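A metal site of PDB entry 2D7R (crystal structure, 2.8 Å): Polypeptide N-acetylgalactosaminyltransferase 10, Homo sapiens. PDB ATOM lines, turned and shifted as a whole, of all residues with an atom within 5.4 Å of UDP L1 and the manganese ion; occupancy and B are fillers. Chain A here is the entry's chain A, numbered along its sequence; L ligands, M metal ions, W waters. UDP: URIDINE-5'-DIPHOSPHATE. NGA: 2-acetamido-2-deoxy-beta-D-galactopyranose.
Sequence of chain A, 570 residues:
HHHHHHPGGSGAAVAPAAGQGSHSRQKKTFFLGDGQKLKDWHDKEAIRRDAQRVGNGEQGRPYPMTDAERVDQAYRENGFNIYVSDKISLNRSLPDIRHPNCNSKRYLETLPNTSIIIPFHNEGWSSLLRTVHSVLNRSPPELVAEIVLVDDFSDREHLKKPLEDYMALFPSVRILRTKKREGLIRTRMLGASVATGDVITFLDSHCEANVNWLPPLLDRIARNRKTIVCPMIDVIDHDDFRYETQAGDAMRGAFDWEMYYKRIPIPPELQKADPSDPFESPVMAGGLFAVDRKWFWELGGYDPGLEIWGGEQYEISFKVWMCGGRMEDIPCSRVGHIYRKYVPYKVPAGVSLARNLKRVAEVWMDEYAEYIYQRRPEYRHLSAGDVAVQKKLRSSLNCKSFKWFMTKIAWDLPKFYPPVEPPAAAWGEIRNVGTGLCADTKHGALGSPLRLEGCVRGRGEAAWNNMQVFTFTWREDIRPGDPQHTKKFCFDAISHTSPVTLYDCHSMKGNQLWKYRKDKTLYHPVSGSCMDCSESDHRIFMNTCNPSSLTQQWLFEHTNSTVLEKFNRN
Within 4 Å of the manganese ion: Asp 204, His 206 and His 337. The nearest printed residue that does not touch the manganese ion is Ile 338 (4.4 Å).
Water W1 is bound to the manganese ion, 2.1 Å away. The manganese ion is bound by OD2 of Asp 204, 2.1 Å away. O3B of UDP L1 binds the manganese ion (2.2 Å). The manganese ion is bound by an oxygen (O1A) of UDP L1 (2.3 Å). The manganese ion is bound by NE2 of His 337, at 2.3 Å. The manganese ion is bound by NE2 of His 206 (2.3 Å).
The backbone NH of Leu 184 sits close to a nitrogen (N3) of UDP L1 (3.5 Å). Residues that only touch UDP L1: Phe 120, Gly 183 and Ile 308. Hydrophobic or aromatic side chains within 4 Å of UDP L1: Pro 119, Phe 120, His 121, Leu 184, His 206, Ile 308, Trp 309, His 337 and Tyr 345. Within 4 Å of UDP L1: Pro 119, Phe 120, His 121, Glu 123, Asp 152, Arg 181, Gly 183, Leu 184, Asp 204, Ser 205, His 206, Ile 308, Trp 309, His 337, Arg 340 and Tyr 345. Along chain A the residues within 4 Å of UDP L1 span positions 119 to 345. The nearest printed residue that does not touch UDP L1 is Thr 187 (4.04 Å).
O3B of UDP L1 sits close to N2 of NGA L2, at 3.3 Å.
ND1 of His 206 sits close to OE2 of Glu 123 (3.4 Å). The backbone carbonyl oxygen (O) of His 206 lies within hydrogen-bond range of the backbone NH (N) of Ile 338, 3.1 Å away. OE1 of Glu 123 is in salt-bridge range of NH2 of Arg 340 (3.1 Å). The guanidinium group of Arg 181 is in salt-bridge range of the side-chain carboxylate of Asp 152, at 3.3 Å. The backbone carbonyl oxygen (O) of Phe 120 sits at hydrogen-bond distance from the backbone NH (N) of Asp 152 (2.8 Å). The backbone NH (N) of Gly 183 is in hydrogen-bond range of the side-chain carboxylate (OD2) of Asp 152, 2.9 Å away. A ring nitrogen (ND1) of His 121 sits close to the guanidinium group (NE) of Arg 181 (3.3 Å). The backbone NH (N) of Leu 184 lies within hydrogen-bond range of the backbone carbonyl oxygen (O) of Ile 308 (3.1 Å).
Water W1 lies within hydrogen-bond range of O2B of UDP L1 (2.9 Å), O of Ile 338 (3.0 Å) and NE of Arg 340 (3.5 Å). Water W2 bridges the backbone NH of Arg 340 (3.0 Å) and an oxygen (O2B) of UDP L1 (3.0 Å).
O of Pro 119 lies within hydrogen-bond range of O3' of UDP L1, 2.5 Å away. The side-chain carboxylate (OE1) of Glu 123 sits at hydrogen-bond distance from an oxygen (O2') of UDP L1 (2.7 Å). The side-chain carboxylate (OD2) of Asp 152 lies within hydrogen-bond range of a nitrogen (N3) of UDP L1. The backbone NH (N) of Ser 205 lies within hydrogen-bond range of an oxygen (O3') of UDP L1 (3.0 Å). OG of Ser 205 lies within hydrogen-bond range of O3' of UDP L1, at 2.8 Å. OH of Tyr 345 sits at hydrogen-bond distance from O2A of UDP L1 (2.9 Å). NH2 of Arg 181 sits at hydrogen-bond distance from O4 of UDP L1. An oxygen (O1B) of UDP L1 sits at hydrogen-bond distance from the indole nitrogen of Trp 309. O2' of UDP L1 lies within hydrogen-bond range of N of His 121, 3.1 Å away. The guanidinium group of Arg 340 lies within salt-bridge range of an oxygen (O2A) of UDP L1. The side-chain carboxylate of Asp 204 lies within hydrogen-bond range of an oxygen (O3) of NGA L2, 3.2 Å away.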
ATOM      1  N   ILE A 118      24.155  -9.265  22.410  1.00  0.00           N
ATOM      2  CA  ILE A 118      25.385  -9.566  23.150  1.00  0.00           C
ATOM      3  C   ILE A 118      25.330  -9.316  24.663  1.00  0.00           C
ATOM      4  O   ILE A 118      25.343  -8.154  25.121  1.00  0.00           O
ATOM      5  CB  ILE A 118      26.595  -8.744  22.638  1.00  0.00           C
ATOM      6  CG1 ILE A 118      26.809  -8.970  21.134  1.00  0.00           C
ATOM      7  CG2 ILE A 118      27.845  -9.163  23.406  1.00  0.00           C
ATOM      8  CD1 ILE A 118      27.889  -8.073  20.515  1.00  0.00           C
ATOM      9  N   PRO A 119      25.280 -10.390  25.466  1.00  0.00           N
ATOM     10  CA  PRO A 119      25.234 -10.280  26.928  1.00  0.00           C
ATOM     11  C   PRO A 119      26.645 -10.161  27.499  1.00  0.00           C
ATOM     12  O   PRO A 119      27.556 -10.905  27.104  1.00  0.00           O
ATOM     13  CB  PRO A 119      24.567 -11.592  27.337  1.00  0.00           C
ATOM     14  CG  PRO A 119      25.157 -12.527  26.387  1.00  0.00           C
ATOM     15  CD  PRO A 119      25.023 -11.770  25.067  1.00  0.00           C
ATOM     16  N   PHE A 120      26.848  -9.233  28.421  1.00  0.00           N
ATOM     17  CA  PHE A 120      28.174  -9.095  29.020  1.00  0.00           C
ATOM     18  C   PHE A 120      28.127  -8.758  30.500  1.00  0.00           C
ATOM     19  O   PHE A 120      27.174  -8.152  30.986  1.00  0.00           O
ATOM     20  CB  PHE A 120      28.991  -8.052  28.253  1.00  0.00           C
ATOM     21  CG  PHE A 120      28.542  -6.645  28.460  1.00  0.00           C
ATOM     22  CD1 PHE A 120      29.037  -5.880  29.518  1.00  0.00           C
ATOM     23  CD2 PHE A 120      27.654  -6.055  27.569  1.00  0.00           C
ATOM     24  CE1 PHE A 120      28.646  -4.549  29.690  1.00  0.00           C
ATOM     25  CE2 PHE A 120      27.245  -4.716  27.726  1.00  0.00           C
ATOM     26  CZ  PHE A 120      27.747  -3.962  28.790  1.00  0.00           C
ATOM     27  N   HIS A 121      29.167  -9.159  31.209  1.00  0.00           N
ATOM     28  CA  HIS A 121      29.268  -8.905  32.629  1.00  0.00           C
ATOM     29  C   HIS A 121      30.720  -8.596  32.941  1.00  0.00           C
ATOM     30  O   HIS A 121      31.566  -9.474  32.933  1.00  0.00           O
ATOM     31  CB  HIS A 121      28.818 -10.127  33.422  1.00  0.00           C
ATOM     32  CG  HIS A 121      28.960  -9.960  34.904  1.00  0.00           C
ATOM     33  ND1 HIS A 121      28.136  -9.148  35.647  1.00  0.00           N
ATOM     34  CD2 HIS A 121      29.871 -10.470  35.767  1.00  0.00           C
ATOM     35  CE1 HIS A 121      28.532  -9.152  36.909  1.00  0.00           C
ATOM     36  NE2 HIS A 121      29.583  -9.942  37.010  1.00  0.00           N
ATOM     37  N   GLU A 123      32.950  -7.183  31.232  1.00  0.00           N
ATOM     38  CA  GLU A 123      33.825  -7.578  30.171  1.00  0.00           C
ATOM     39  C   GLU A 123      34.885  -6.491  29.908  1.00  0.00           C
ATOM     40  O   GLU A 123      34.668  -5.319  30.184  1.00  0.00           O
ATOM     41  CB  GLU A 123      32.988  -7.878  28.921  1.00  0.00           C
ATOM     42  CG  GLU A 123      33.586  -9.006  28.056  1.00  0.00           C
ATOM     43  CD  GLU A 123      33.720 -10.322  28.799  1.00  0.00           C
ATOM     44  OE1 GLU A 123      32.683 -10.981  29.011  1.00  0.00           O
ATOM     45  OE2 GLU A 123      34.855 -10.674  29.198  1.00  0.00           O
ATOM     46  N   VAL A 150      23.856  -6.086  26.172  1.00  0.00           N
ATOM     47  CA  VAL A 150      23.075  -6.193  27.372  1.00  0.00           C
ATOM     48  C   VAL A 150      24.001  -6.322  28.569  1.00  0.00           C
ATOM     49  O   VAL A 150      24.654  -7.347  28.764  1.00  0.00           O
ATOM     50  CB  VAL A 150      22.101  -7.417  27.309  1.00  0.00           C
ATOM     51  CG1 VAL A 150      21.028  -7.294  28.381  1.00  0.00           C
ATOM     52  CG2 VAL A 150      21.443  -7.484  25.914  1.00  0.00           C
ATOM     53  N   ASP A 152      24.836  -7.046  32.140  1.00  0.00           N
ATOM     54  CA  ASP A 152      24.291  -7.812  33.241  1.00  0.00           C
ATOM     55  C   ASP A 152      24.842  -7.293  34.550  1.00  0.00           C
ATOM     56  O   ASP A 152      25.698  -7.907  35.165  1.00  0.00           O
ATOM     57  CB  ASP A 152      24.619  -9.303  33.075  1.00  0.00           C
ATOM     58  CG  ASP A 152      24.012 -10.146  34.182  1.00  0.00           C
ATOM     59  OD1 ASP A 152      23.001  -9.728  34.783  1.00  0.00           O
ATOM     60  OD2 ASP A 152      24.543 -11.245  34.453  1.00  0.00           O
ATOM     61  N   ARG A 181      21.904  -8.599  39.036  1.00  0.00           N
ATOM     62  CA  ARG A 181      22.587  -9.724  38.416  1.00  0.00           C
ATOM     63  C   ARG A 181      21.558 -10.773  37.987  1.00  0.00           C
ATOM     64  O   ARG A 181      20.889 -11.358  38.838  1.00  0.00           O
ATOM     65  CB  ARG A 181      23.600 -10.337  39.396  1.00  0.00           C
ATOM     66  CG  ARG A 181      24.564 -11.329  38.771  1.00  0.00           C
ATOM     67  CD  ARG A 181      25.444 -10.656  37.707  1.00  0.00           C
ATOM     68  NE  ARG A 181      26.431 -11.567  37.141  1.00  0.00           N
ATOM     69  CZ  ARG A 181      27.340 -12.241  37.854  1.00  0.00           C
ATOM     70  NH1 ARG A 181      27.394 -12.119  39.165  1.00  0.00           N
ATOM     71  NH2 ARG A 181      28.184 -13.060  37.243  1.00  0.00           N
ATOM     72  N   GLY A 183      22.364 -13.095  35.124  1.00  0.00           N
ATOM     73  CA  GLY A 183      23.140 -14.230  34.670  1.00  0.00           C
ATOM     74  C   GLY A 183      23.021 -14.249  33.168  1.00  0.00           C
ATOM     75  O   GLY A 183      22.210 -13.486  32.613  1.00  0.00           O
ATOM     76  N   LEU A 184      23.796 -15.102  32.502  1.00  0.00           N
ATOM     77  CA  LEU A 184      23.768 -15.133  31.048  1.00  0.00           C
ATOM     78  C   LEU A 184      22.433 -15.564  30.438  1.00  0.00           C
ATOM     79  O   LEU A 184      21.969 -14.959  29.472  1.00  0.00           O
ATOM     80  CB  LEU A 184      24.938 -15.973  30.517  1.00  0.00           C
ATOM     81  CG  LEU A 184      25.033 -17.500  30.616  1.00  0.00           C
ATOM     82  CD1 LEU A 184      24.262 -18.188  29.480  1.00  0.00           C
ATOM     83  CD2 LEU A 184      26.485 -17.893  30.569  1.00  0.00           C
ATOM     84  N   THR A 187      19.888 -12.799  30.959  1.00  0.00           N
ATOM     85  CA  THR A 187      20.347 -11.617  30.249  1.00  0.00           C
ATOM     86  C   THR A 187      20.054 -11.779  28.755  1.00  0.00           C
ATOM     87  O   THR A 187      19.605 -10.843  28.099  1.00  0.00           O
ATOM     88  CB  THR A 187      21.863 -11.373  30.442  1.00  0.00           C
ATOM     89  OG1 THR A 187      22.148 -11.152  31.836  1.00  0.00           O
ATOM     90  CG2 THR A 187      22.304 -10.156  29.649  1.00  0.00           C
ATOM     91  N   ARG A 188      20.303 -12.965  28.222  1.00  0.00           N
ATOM     92  CA  ARG A 188      20.053 -13.189  26.818  1.00  0.00           C
ATOM     93  C   ARG A 188      18.569 -13.145  26.523  1.00  0.00           C
ATOM     94  O   ARG A 188      18.163 -12.847  25.396  1.00  0.00           O
ATOM     95  CB  ARG A 188      20.656 -14.518  26.356  1.00  0.00           C
ATOM     96  CG  ARG A 188      22.161 -14.491  26.376  1.00  0.00           C
ATOM     97  CD  ARG A 188      22.761 -15.346  25.295  1.00  0.00           C
ATOM     98  NE  ARG A 188      22.505 -16.751  25.530  1.00  0.00           N
ATOM     99  CZ  ARG A 188      23.466 -17.669  25.641  1.00  0.00           C
ATOM    100  NH1 ARG A 188      24.747 -17.325  25.537  1.00  0.00           N
ATOM    101  NH2 ARG A 188      23.128 -18.941  25.858  1.00  0.00           N
ATOM    102  N   LEU A 203      25.782 -13.763  20.435  1.00  0.00           N
ATOM    103  CA  LEU A 203      27.250 -13.799  20.362  1.00  0.00           C
ATOM    104  C   LEU A 203      27.778 -13.501  21.757  1.00  0.00           C
ATOM    105  O   LEU A 203      27.087 -12.891  22.549  1.00  0.00           O
ATOM    106  CB  LEU A 203      27.742 -12.713  19.425  1.00  0.00           C
ATOM    107  CG  LEU A 203      28.221 -12.975  18.001  1.00  0.00           C
ATOM    108  CD1 LEU A 203      27.360 -13.960  17.279  1.00  0.00           C
ATOM    109  CD2 LEU A 203      28.226 -11.639  17.281  1.00  0.00           C
ATOM    110  N   ASP A 204      28.993 -13.938  22.080  1.00  0.00           N
ATOM    111  CA  ASP A 204      29.551 -13.630  23.394  1.00  0.00           C
ATOM    112  C   ASP A 204      30.226 -12.291  23.257  1.00  0.00           C
ATOM    113  O   ASP A 204      30.438 -11.827  22.141  1.00  0.00           O
ATOM    114  CB  ASP A 204      30.571 -14.677  23.818  1.00  0.00           C
ATOM    115  CG  ASP A 204      29.980 -15.747  24.743  1.00  0.00           C
ATOM    116  OD1 ASP A 204      28.744 -15.755  24.968  1.00  0.00           O
ATOM    117  OD2 ASP A 204      30.765 -16.582  25.242  1.00  0.00           O
ATOM    118  N   SER A 205      30.566 -11.652  24.365  1.00  0.00           N
ATOM    119  CA  SER A 205      31.188 -10.327  24.291  1.00  0.00           C
ATOM    120  C   SER A 205      32.669 -10.294  23.966  1.00  0.00           C
ATOM    121  O   SER A 205      33.310  -9.260  24.119  1.00  0.00           O
ATOM    122  CB  SER A 205      30.963  -9.580  25.587  1.00  0.00           C
ATOM    123  OG  SER A 205      31.377 -10.391  26.660  1.00  0.00           O
ATOM    124  N   HIS A 206      33.203 -11.418  23.525  1.00  0.00           N
ATOM    125  CA  HIS A 206      34.636 -11.516  23.178  1.00  0.00           C
ATOM    126  C   HIS A 206      34.795 -12.441  21.990  1.00  0.00           C
ATOM    127  O   HIS A 206      35.437 -13.490  22.086  1.00  0.00           O
ATOM    128  CB  HIS A 206      35.443 -12.051  24.372  1.00  0.00           C
ATOM    129  CG  HIS A 206      34.684 -13.009  25.231  1.00  0.00           C
ATOM    130  ND1 HIS A 206      34.349 -12.727  26.537  1.00  0.00           N
ATOM    131  CD2 HIS A 206      34.136 -14.210  24.956  1.00  0.00           C
ATOM    132  CE1 HIS A 206      33.617 -13.716  27.029  1.00  0.00           C
ATOM    133  NE2 HIS A 206      33.474 -14.631  26.084  1.00  0.00           N
ATOM    134  N   ILE A 308      23.409 -18.518  36.683  1.00  0.00           N
ATOM    135  CA  ILE A 308      24.427 -17.675  36.067  1.00  0.00           C
ATOM    136  C   ILE A 308      25.101 -18.207  34.819  1.00  0.00           C
ATOM    137  O   ILE A 308      25.314 -17.466  33.862  1.00  0.00           O
ATOM    138  CB  ILE A 308      25.559 -17.300  37.089  1.00  0.00           C
ATOM    139  CG1 ILE A 308      25.014 -16.375  38.174  1.00  0.00           C
ATOM    140  CG2 ILE A 308      26.698 -16.584  36.375  1.00  0.00           C
ATOM    141  CD1 ILE A 308      24.481 -17.094  39.381  1.00  0.00           C
ATOM    142  N   TRP A 309      25.388 -19.495  34.804  1.00  0.00           N
ATOM    143  CA  TRP A 309      26.102 -20.096  33.687  1.00  0.00           C
ATOM    144  C   TRP A 309      25.735 -21.577  33.535  1.00  0.00           C
ATOM    145  O   TRP A 309      25.263 -22.213  34.481  1.00  0.00           O
ATOM    146  CB  TRP A 309      27.609 -19.947  33.963  1.00  0.00           C
ATOM    147  CG  TRP A 309      28.510 -20.499  32.917  1.00  0.00           C
ATOM    148  CD1 TRP A 309      29.076 -19.827  31.871  1.00  0.00           C
ATOM    149  CD2 TRP A 309      28.913 -21.864  32.787  1.00  0.00           C
ATOM    150  NE1 TRP A 309      29.810 -20.692  31.095  1.00  0.00           N
ATOM    151  CE2 TRP A 309      29.729 -21.946  31.633  1.00  0.00           C
ATOM    152  CE3 TRP A 309      28.672 -23.024  33.521  1.00  0.00           C
ATOM    153  CZ2 TRP A 309      30.307 -23.151  31.212  1.00  0.00           C
ATOM    154  CZ3 TRP A 309      29.250 -24.228  33.100  1.00  0.00           C
ATOM    155  CH2 TRP A 309      30.048 -24.274  31.950  1.00  0.00           C
ATOM    156  N   HIS A 337      36.239 -16.817  19.125  1.00  0.00           N
ATOM    157  CA  HIS A 337      35.786 -16.685  20.496  1.00  0.00           C
ATOM    158  C   HIS A 337      36.955 -16.912  21.421  1.00  0.00           C
ATOM    159  O   HIS A 337      37.782 -17.787  21.173  1.00  0.00           O
ATOM    160  CB  HIS A 337      34.688 -17.712  20.795  1.00  0.00           C
ATOM    161  CG  HIS A 337      34.299 -17.776  22.236  1.00  0.00           C
ATOM    162  ND1 HIS A 337      34.856 -18.670  23.121  1.00  0.00           N
ATOM    163  CD2 HIS A 337      33.466 -16.990  22.975  1.00  0.00           C
ATOM    164  CE1 HIS A 337      34.388 -18.436  24.332  1.00  0.00           C
ATOM    165  NE2 HIS A 337      33.543 -17.424  24.269  1.00  0.00           N
ATOM    166  N   ILE A 338      37.027 -16.135  22.487  1.00  0.00           N
ATOM    167  CA  ILE A 338      38.131 -16.250  23.438  1.00  0.00           C
ATOM    168  C   ILE A 338      37.732 -17.137  24.575  1.00  0.00           C
ATOM    169  O   ILE A 338      36.972 -16.710  25.423  1.00  0.00           O
ATOM    170  CB  ILE A 338      38.514 -14.901  24.096  1.00  0.00           C
ATOM    171  CG1 ILE A 338      38.751 -13.832  23.050  1.00  0.00           C
ATOM    172  CG2 ILE A 338      39.752 -15.061  24.936  1.00  0.00           C
ATOM    173  CD1 ILE A 338      39.059 -12.459  23.648  1.00  0.00           C
ATOM    174  N   ARG A 340      38.205 -18.530  28.018  1.00  0.00           N
ATOM    175  CA  ARG A 340      38.928 -18.109  29.213  1.00  0.00           C
ATOM    176  C   ARG A 340      39.872 -19.152  29.775  1.00  0.00           C
ATOM    177  O   ARG A 340      39.642 -20.347  29.622  1.00  0.00           O
ATOM    178  CB  ARG A 340      37.949 -17.722  30.320  1.00  0.00           C
ATOM    179  CG  ARG A 340      37.000 -16.603  29.950  1.00  0.00           C
ATOM    180  CD  ARG A 340      35.937 -16.464  30.992  1.00  0.00           C
ATOM    181  NE  ARG A 340      34.823 -15.700  30.463  1.00  0.00           N
ATOM    182  CZ  ARG A 340      34.701 -14.386  30.549  1.00  0.00           C
ATOM    183  NH1 ARG A 340      35.630 -13.672  31.149  1.00  0.00           N
ATOM    184  NH2 ARG A 340      33.634 -13.800  30.024  1.00  0.00           N
ATOM    185  N   TYR A 345      34.640 -13.269  36.909  1.00  0.00           N
ATOM    186  CA  TYR A 345      33.494 -12.795  37.656  1.00  0.00           C
ATOM    187  C   TYR A 345      33.099 -13.709  38.806  1.00  0.00           C
ATOM    188  O   TYR A 345      33.409 -14.904  38.820  1.00  0.00           O
ATOM    189  CB  TYR A 345      32.279 -12.586  36.748  1.00  0.00           C
ATOM    190  CG  TYR A 345      31.914 -13.755  35.889  1.00  0.00           C
ATOM    191  CD1 TYR A 345      32.453 -13.898  34.621  1.00  0.00           C
ATOM    192  CD2 TYR A 345      31.001 -14.708  36.342  1.00  0.00           C
ATOM    193  CE1 TYR A 345      32.101 -14.972  33.805  1.00  0.00           C
ATOM    194  CE2 TYR A 345      30.639 -15.780  35.540  1.00  0.00           C
ATOM    195  CZ  TYR A 345      31.191 -15.906  34.272  1.00  0.00           C
ATOM    196  OH  TYR A 345      30.849 -16.954  33.461  1.00  0.00           O
HETATM  197  N1  UDP L   1      27.760 -13.180  31.106  1.00  0.00           N
HETATM  198  C2  UDP L   1      26.668 -12.477  31.602  1.00  0.00           C
HETATM  199  N3  UDP L   1      26.274 -12.676  32.901  1.00  0.00           N
HETATM  200  C4  UDP L   1      26.939 -13.552  33.720  1.00  0.00           C
HETATM  201  C5  UDP L   1      28.041 -14.274  33.227  1.00  0.00           C
HETATM  202  C6  UDP L   1      28.383 -14.140  31.882  1.00  0.00           C
HETATM  203  O2  UDP L   1      26.047 -11.678  30.911  1.00  0.00           O
HETATM  204  O4  UDP L   1      26.557 -13.699  34.869  1.00  0.00           O
HETATM  205  C1' UDP L   1      28.139 -12.957  29.700  1.00  0.00           C
HETATM  206  C2' UDP L   1      29.625 -12.902  29.412  1.00  0.00           C
HETATM  207  O2' UDP L   1      30.106 -11.574  29.493  1.00  0.00           O
HETATM  208  C3' UDP L   1      29.708 -13.488  28.015  1.00  0.00           C
HETATM  209  C4' UDP L   1      28.531 -14.450  27.937  1.00  0.00           C
HETATM  210  O4' UDP L   1      27.646 -14.063  28.977  1.00  0.00           O
HETATM  211  O3' UDP L   1      29.496 -12.498  27.023  1.00  0.00           O
HETATM  212  C5' UDP L   1      28.894 -15.934  28.095  1.00  0.00           C
HETATM  213  O5' UDP L   1      29.526 -16.183  29.336  1.00  0.00           O
HETATM  214  PA  UDP L   1      31.073 -16.651  29.383  1.00  0.00           P
HETATM  215  O1A UDP L   1      31.850 -16.075  28.267  1.00  0.00           O
HETATM  216  O2A UDP L   1      31.633 -16.299  30.709  1.00  0.00           O
HETATM  217  O3A UDP L   1      30.965 -18.232  29.168  1.00  0.00           O
HETATM  218  PB  UDP L   1      32.080 -19.105  28.418  1.00  0.00           P
HETATM  219  O1B UDP L   1      31.665 -20.506  28.663  1.00  0.00           O
HETATM  220  O2B UDP L   1      33.425 -18.860  28.976  1.00  0.00           O
HETATM  221  O3B UDP L   1      32.159 -18.793  26.965  1.00  0.00           O
HETATM  222  C1  NGA L   2      29.456 -22.408  26.583  1.00  0.00           C
HETATM  223  C2  NGA L   2      29.187 -21.131  25.779  1.00  0.00           C
HETATM  224  C3  NGA L   2      28.797 -20.006  26.749  1.00  0.00           C
HETATM  225  C4  NGA L   2      27.577 -20.428  27.574  1.00  0.00           C
HETATM  226  C5  NGA L   2      27.895 -21.759  28.276  1.00  0.00           C
HETATM  227  C6  NGA L   2      26.651 -22.242  29.016  1.00  0.00           C
HETATM  228  C7  NGA L   2      30.457 -20.846  23.687  1.00  0.00           C
HETATM  229  C8  NGA L   2      31.793 -20.395  23.106  1.00  0.00           C
HETATM  230  N2  NGA L   2      30.381 -20.755  25.012  1.00  0.00           N
HETATM  231  O1  NGA L   2      29.797 -23.481  25.693  1.00  0.00           O
HETATM  232  O3  NGA L   2      28.480 -18.816  26.019  1.00  0.00           O
HETATM  233  O4  NGA L   2      26.440 -20.578  26.720  1.00  0.00           O
HETATM  234  O5  NGA L   2      28.272 -22.767  27.319  1.00  0.00           O
HETATM  235  O6  NGA L   2      26.271 -21.268  29.996  1.00  0.00           O
HETATM  236  O7  NGA L   2      29.550 -21.239  22.953  1.00  0.00           O
HETATM  237 MN    MN M   1      32.637 -16.771  26.251  1.00  0.00          MN
HETATM  238  O   HOH W   1      34.540 -16.881  27.187  1.00  0.00           O
HETATM  239  O   HOH W   2      35.869 -20.439  28.084  1.00  0.00           O
